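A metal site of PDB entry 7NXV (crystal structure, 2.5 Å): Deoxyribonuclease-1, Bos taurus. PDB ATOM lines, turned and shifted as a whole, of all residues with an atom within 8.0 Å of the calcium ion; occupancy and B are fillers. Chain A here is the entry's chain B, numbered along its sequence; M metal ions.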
ATOM      1  N   LEU A  71       6.106 -30.341   4.709  1.00  0.00           N
ATOM      2  CA  LEU A  71       7.599 -30.380   4.712  1.00  0.00           C
ATOM      3  C   LEU A  71       8.098 -31.050   6.007  1.00  0.00           C
ATOM      4  O   LEU A  71       7.514 -30.775   7.080  1.00  0.00           O
ATOM      5  CB  LEU A  71       8.135 -28.954   4.620  1.00  0.00           C
ATOM      6  CG  LEU A  71       7.611 -28.132   3.443  1.00  0.00           C
ATOM      7  CD1 LEU A  71       8.114 -26.694   3.520  1.00  0.00           C
ATOM      8  CD2 LEU A  71       8.008 -28.757   2.115  1.00  0.00           C
ATOM      9  N   GLY A  72       9.145 -31.872   5.892  1.00  0.00           N
ATOM     10  CA  GLY A  72       9.771 -32.585   7.024  1.00  0.00           C
ATOM     11  C   GLY A  72      10.555 -33.801   6.550  1.00  0.00           C
ATOM     12  O   GLY A  72      10.161 -34.407   5.537  1.00  0.00           O
ATOM     13  N   ARG A  73      11.616 -34.154   7.287  1.00  0.00           N
ATOM     14  CA  ARG A  73      12.495 -35.323   6.983  1.00  0.00           C
ATOM     15  C   ARG A  73      11.787 -36.624   7.401  1.00  0.00           C
ATOM     16  O   ARG A  73      12.122 -37.680   6.840  1.00  0.00           O
ATOM     17  CB  ARG A  73      13.831 -35.195   7.712  1.00  0.00           C
ATOM     18  CG  ARG A  73      14.724 -34.070   7.182  1.00  0.00           C
ATOM     19  CD  ARG A  73      16.169 -34.245   7.617  1.00  0.00           C
ATOM     20  NE  ARG A  73      16.988 -33.065   7.396  1.00  0.00           N
ATOM     21  CZ  ARG A  73      17.128 -32.043   8.241  1.00  0.00           C
ATOM     22  NH1 ARG A  73      17.902 -31.026   7.914  1.00  0.00           N
ATOM     23  NH2 ARG A  73      16.494 -32.037   9.411  1.00  0.00           N
ATOM     24  N   TYR A  97      12.984 -23.435  -1.512  1.00  0.00           N
ATOM     25  CA  TYR A  97      14.466 -23.460  -1.483  1.00  0.00           C
ATOM     26  C   TYR A  97      14.944 -24.904  -1.668  1.00  0.00           C
ATOM     27  O   TYR A  97      14.432 -25.812  -0.973  1.00  0.00           O
ATOM     28  CB  TYR A  97      15.034 -22.872  -0.185  1.00  0.00           C
ATOM     29  CG  TYR A  97      16.535 -22.919  -0.106  1.00  0.00           C
ATOM     30  CD1 TYR A  97      17.319 -22.130  -0.926  1.00  0.00           C
ATOM     31  CD2 TYR A  97      17.183 -23.777   0.771  1.00  0.00           C
ATOM     32  CE1 TYR A  97      18.699 -22.171  -0.868  1.00  0.00           C
ATOM     33  CE2 TYR A  97      18.570 -23.833   0.839  1.00  0.00           C
ATOM     34  CZ  TYR A  97      19.334 -23.033   0.012  1.00  0.00           C
ATOM     35  OH  TYR A  97      20.696 -23.070   0.067  1.00  0.00           O
ATOM     36  N   ASP A  98      15.879 -25.126  -2.602  1.00  0.00           N
ATOM     37  CA  ASP A  98      16.600 -26.403  -2.787  1.00  0.00           C
ATOM     38  C   ASP A  98      17.695 -26.470  -1.727  1.00  0.00           C
ATOM     39  O   ASP A  98      18.723 -25.790  -1.883  1.00  0.00           O
ATOM     40  CB  ASP A  98      17.153 -26.535  -4.212  1.00  0.00           C
ATOM     41  CG  ASP A  98      17.676 -27.913  -4.555  1.00  0.00           C
ATOM     42  OD1 ASP A  98      18.102 -28.629  -3.627  1.00  0.00           O
ATOM     43  OD2 ASP A  98      17.651 -28.271  -5.744  1.00  0.00           O
ATOM     44  N   ASP A  99      17.454 -27.248  -0.663  1.00  0.00           N
ATOM     45  CA  ASP A  99      18.346 -27.362   0.525  1.00  0.00           C
ATOM     46  C   ASP A  99      19.282 -28.559   0.344  1.00  0.00           C
ATOM     47  O   ASP A  99      19.990 -28.895   1.304  1.00  0.00           O
ATOM     48  CB  ASP A  99      17.535 -27.445   1.818  1.00  0.00           C
ATOM     49  CG  ASP A  99      16.764 -28.733   2.020  1.00  0.00           C
ATOM     50  OD1 ASP A  99      16.526 -29.098   3.183  1.00  0.00           O
ATOM     51  OD2 ASP A  99      16.376 -29.363   1.006  1.00  0.00           O
ATOM     52  N   GLY A 100      19.294 -29.169  -0.854  1.00  0.00           N
ATOM     53  CA  GLY A 100      20.205 -30.272  -1.218  1.00  0.00           C
ATOM     54  C   GLY A 100      19.508 -31.618  -1.164  1.00  0.00           C
ATOM     55  O   GLY A 100      18.265 -31.653  -1.271  1.00  0.00           O
ATOM     56  N   CYS A 101      20.286 -32.680  -0.957  1.00  0.00           N
ATOM     57  CA  CYS A 101      19.887 -34.097  -1.128  1.00  0.00           C
ATOM     58  C   CYS A 101      19.422 -34.692   0.214  1.00  0.00           C
ATOM     59  O   CYS A 101      20.284 -34.891   1.097  1.00  0.00           O
ATOM     60  CB  CYS A 101      21.061 -34.873  -1.726  1.00  0.00           C
ATOM     61  SG  CYS A 101      20.809 -36.657  -1.846  1.00  0.00           S
ATOM     62  N   GLU A 102      18.112 -34.924   0.355  1.00  0.00           N
ATOM     63  CA  GLU A 102      17.462 -35.495   1.577  1.00  0.00           C
ATOM     64  C   GLU A 102      17.930 -36.934   1.795  1.00  0.00           C
ATOM     65  O   GLU A 102      18.214 -37.288   2.958  1.00  0.00           O
ATOM     66  CB  GLU A 102      15.935 -35.475   1.458  1.00  0.00           C
ATOM     67  CG  GLU A 102      15.258 -34.299   2.139  1.00  0.00           C
ATOM     68  CD  GLU A 102      15.138 -33.023   1.312  1.00  0.00           C
ATOM     69  OE1 GLU A 102      15.332 -31.921   1.881  1.00  0.00           O
ATOM     70  OE2 GLU A 102      14.824 -33.121   0.109  1.00  0.00           O
ATOM     71  N   ASN A 106      22.141 -34.717   3.672  1.00  0.00           N
ATOM     72  CA  ASN A 106      22.920 -33.464   3.488  1.00  0.00           C
ATOM     73  C   ASN A 106      22.004 -32.231   3.446  1.00  0.00           C
ATOM     74  O   ASN A 106      22.555 -31.109   3.490  1.00  0.00           O
ATOM     75  CB  ASN A 106      23.737 -33.486   2.192  1.00  0.00           C
ATOM     76  CG  ASN A 106      24.875 -34.489   2.223  1.00  0.00           C
ATOM     77  OD1 ASN A 106      25.390 -34.816   3.288  1.00  0.00           O
ATOM     78  ND2 ASN A 106      25.267 -34.962   1.056  1.00  0.00           N
ATOM     79  N   ASP A 107      20.686 -32.409   3.335  1.00  0.00           N
ATOM     80  CA  ASP A 107      19.690 -31.308   3.256  1.00  0.00           C
ATOM     81  C   ASP A 107      19.800 -30.428   4.509  1.00  0.00           C
ATOM     82  O   ASP A 107      19.798 -30.982   5.620  1.00  0.00           O
ATOM     83  CB  ASP A 107      18.278 -31.856   3.039  1.00  0.00           C
ATOM     84  CG  ASP A 107      17.781 -32.722   4.188  1.00  0.00           C
ATOM     85  OD1 ASP A 107      16.735 -32.375   4.762  1.00  0.00           O
ATOM     86  OD2 ASP A 107      18.462 -33.720   4.495  1.00  0.00           O
ATOM     87  N   SER A 108      19.902 -29.111   4.333  1.00  0.00           N
ATOM     88  CA  SER A 108      20.279 -28.130   5.386  1.00  0.00           C
ATOM     89  C   SER A 108      19.082 -27.754   6.268  1.00  0.00           C
ATOM     90  O   SER A 108      19.321 -27.252   7.387  1.00  0.00           O
ATOM     91  CB  SER A 108      20.917 -26.898   4.786  1.00  0.00           C
ATOM     92  OG  SER A 108      20.156 -26.379   3.711  1.00  0.00           O
ATOM     93  N   PHE A 109      17.842 -27.984   5.811  1.00  0.00           N
ATOM     94  CA  PHE A 109      16.595 -27.594   6.526  1.00  0.00           C
ATOM     95  C   PHE A 109      15.646 -28.789   6.645  1.00  0.00           C
ATOM     96  O   PHE A 109      15.489 -29.517   5.652  1.00  0.00           O
ATOM     97  CB  PHE A 109      15.871 -26.467   5.782  1.00  0.00           C
ATOM     98  CG  PHE A 109      16.598 -25.144   5.787  1.00  0.00           C
ATOM     99  CD1 PHE A 109      17.300 -24.713   4.666  1.00  0.00           C
ATOM    100  CD2 PHE A 109      16.553 -24.329   6.906  1.00  0.00           C
ATOM    101  CE1 PHE A 109      17.954 -23.495   4.684  1.00  0.00           C
ATOM    102  CE2 PHE A 109      17.210 -23.106   6.910  1.00  0.00           C
ATOM    103  CZ  PHE A 109      17.919 -22.691   5.801  1.00  0.00           C
ATOM    104  N   SER A 110      15.023 -28.962   7.815  1.00  0.00           N
ATOM    105  CA  SER A 110      13.934 -29.952   8.020  1.00  0.00           C
ATOM    106  C   SER A 110      12.700 -29.488   7.240  1.00  0.00           C
ATOM    107  O   SER A 110      12.090 -30.320   6.534  1.00  0.00           O
ATOM    108  CB  SER A 110      13.624 -30.161   9.487  1.00  0.00           C
ATOM    109  OG  SER A 110      12.711 -29.192   9.960  1.00  0.00           O
ATOM    110  N   ARG A 111      12.377 -28.189   7.320  1.00  0.00           N
ATOM    111  CA  ARG A 111      11.303 -27.521   6.553  1.00  0.00           C
ATOM    112  C   ARG A 111      11.923 -26.461   5.631  1.00  0.00           C
ATOM    113  O   ARG A 111      12.130 -25.323   6.093  1.00  0.00           O
ATOM    114  CB  ARG A 111      10.274 -26.907   7.510  1.00  0.00           C
ATOM    115  CG  ARG A 111       9.518 -27.930   8.334  1.00  0.00           C
ATOM    116  CD  ARG A 111       8.698 -27.279   9.426  1.00  0.00           C
ATOM    117  NE  ARG A 111       9.515 -26.874  10.560  1.00  0.00           N
ATOM    118  CZ  ARG A 111       9.875 -27.653  11.574  1.00  0.00           C
ATOM    119  NH1 ARG A 111       9.502 -28.919  11.616  1.00  0.00           N
ATOM    120  NH2 ARG A 111      10.626 -27.169  12.547  1.00  0.00           N
ATOM    121  N   GLU A 112      12.221 -26.840   4.382  1.00  0.00           N
ATOM    122  CA  GLU A 112      12.884 -25.970   3.369  1.00  0.00           C
ATOM    123  C   GLU A 112      12.097 -24.662   3.236  1.00  0.00           C
ATOM    124  O   GLU A 112      10.897 -24.690   2.962  1.00  0.00           O
ATOM    125  CB  GLU A 112      12.931 -26.639   1.992  1.00  0.00           C
ATOM    126  CG  GLU A 112      13.529 -28.025   1.993  1.00  0.00           C
ATOM    127  CD  GLU A 112      12.529 -29.165   2.039  1.00  0.00           C
ATOM    128  OE1 GLU A 112      11.375 -28.966   1.609  1.00  0.00           O
ATOM    129  OE2 GLU A 112      12.908 -30.261   2.502  1.00  0.00           O
ATOM    130  N   PRO A 113      12.749 -23.485   3.400  1.00  0.00           N
ATOM    131  CA  PRO A 113      12.071 -22.207   3.245  1.00  0.00           C
ATOM    132  C   PRO A 113      11.239 -22.083   1.958  1.00  0.00           C
ATOM    133  O   PRO A 113      11.737 -22.416   0.899  1.00  0.00           O
ATOM    134  CB  PRO A 113      13.224 -21.199   3.208  1.00  0.00           C
ATOM    135  CG  PRO A 113      14.299 -21.851   4.051  1.00  0.00           C
ATOM    136  CD  PRO A 113      14.167 -23.332   3.760  1.00  0.00           C
ATOM    137  N   GLU A 143      20.514 -24.097  10.932  1.00  0.00           N
ATOM    138  CA  GLU A 143      19.410 -23.725  10.008  1.00  0.00           C
ATOM    139  C   GLU A 143      19.384 -22.193   9.831  1.00  0.00           C
ATOM    140  O   GLU A 143      19.298 -21.755   8.672  1.00  0.00           O
ATOM    141  CB  GLU A 143      18.082 -24.317  10.489  1.00  0.00           C
ATOM    142  CG  GLU A 143      17.964 -25.807  10.213  1.00  0.00           C
ATOM    143  CD  GLU A 143      16.583 -26.427  10.392  1.00  0.00           C
ATOM    144  OE1 GLU A 143      15.635 -25.701  10.713  1.00  0.00           O
ATOM    145  OE2 GLU A 143      16.455 -27.664  10.201  1.00  0.00           O
HETATM  146 CA    CA M   1      14.642 -30.860   4.072  1.00  0.00          CA
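The backbone carbonyl oxygen (O) of Phe 109 binds the calcium ion (2.2 Å). OE2 of Glu 112 binds the calcium ion, at 2.4 Å. The calcium ion is bound by the side-chain carboxylate (OE1) of Glu 102, at 2.5 Å. The calcium ion is bound by OD1 of Asp 107, at 2.7 Å. The calcium ion is bound by the side-chain carboxylate (OD1) of Asp 99, 2.7 Å away. The calcium ion has five donor atoms within binding distance.
O of Ser 110 touches the calcium ion, 3.6 Å away. The nearest printed residue that does not touch the calcium ion is Arg 73 (4.5 Å).
The guanidinium group (NE) of Arg 73 lies within salt-bridge range of the side-chain carboxylate (OD2) of Asp 107 (3.3 Å). N of Asp 107 sits at hydrogen-bond distance from O of Cys 101 (3.4 Å). The backbone NH of Ser 108 lies within hydrogen-bond range of the backbone carbonyl oxygen of Asp 99. The backbone carbonyl oxygen (O) of Ser 110 lies close to the backbone NH (N) of Gly 72 (3.4 Å). The backbone NH (N) of Ser 110 is in hydrogen-bond range of the side-chain carboxylate (OE2) of Glu 143, at 3.1 Å.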
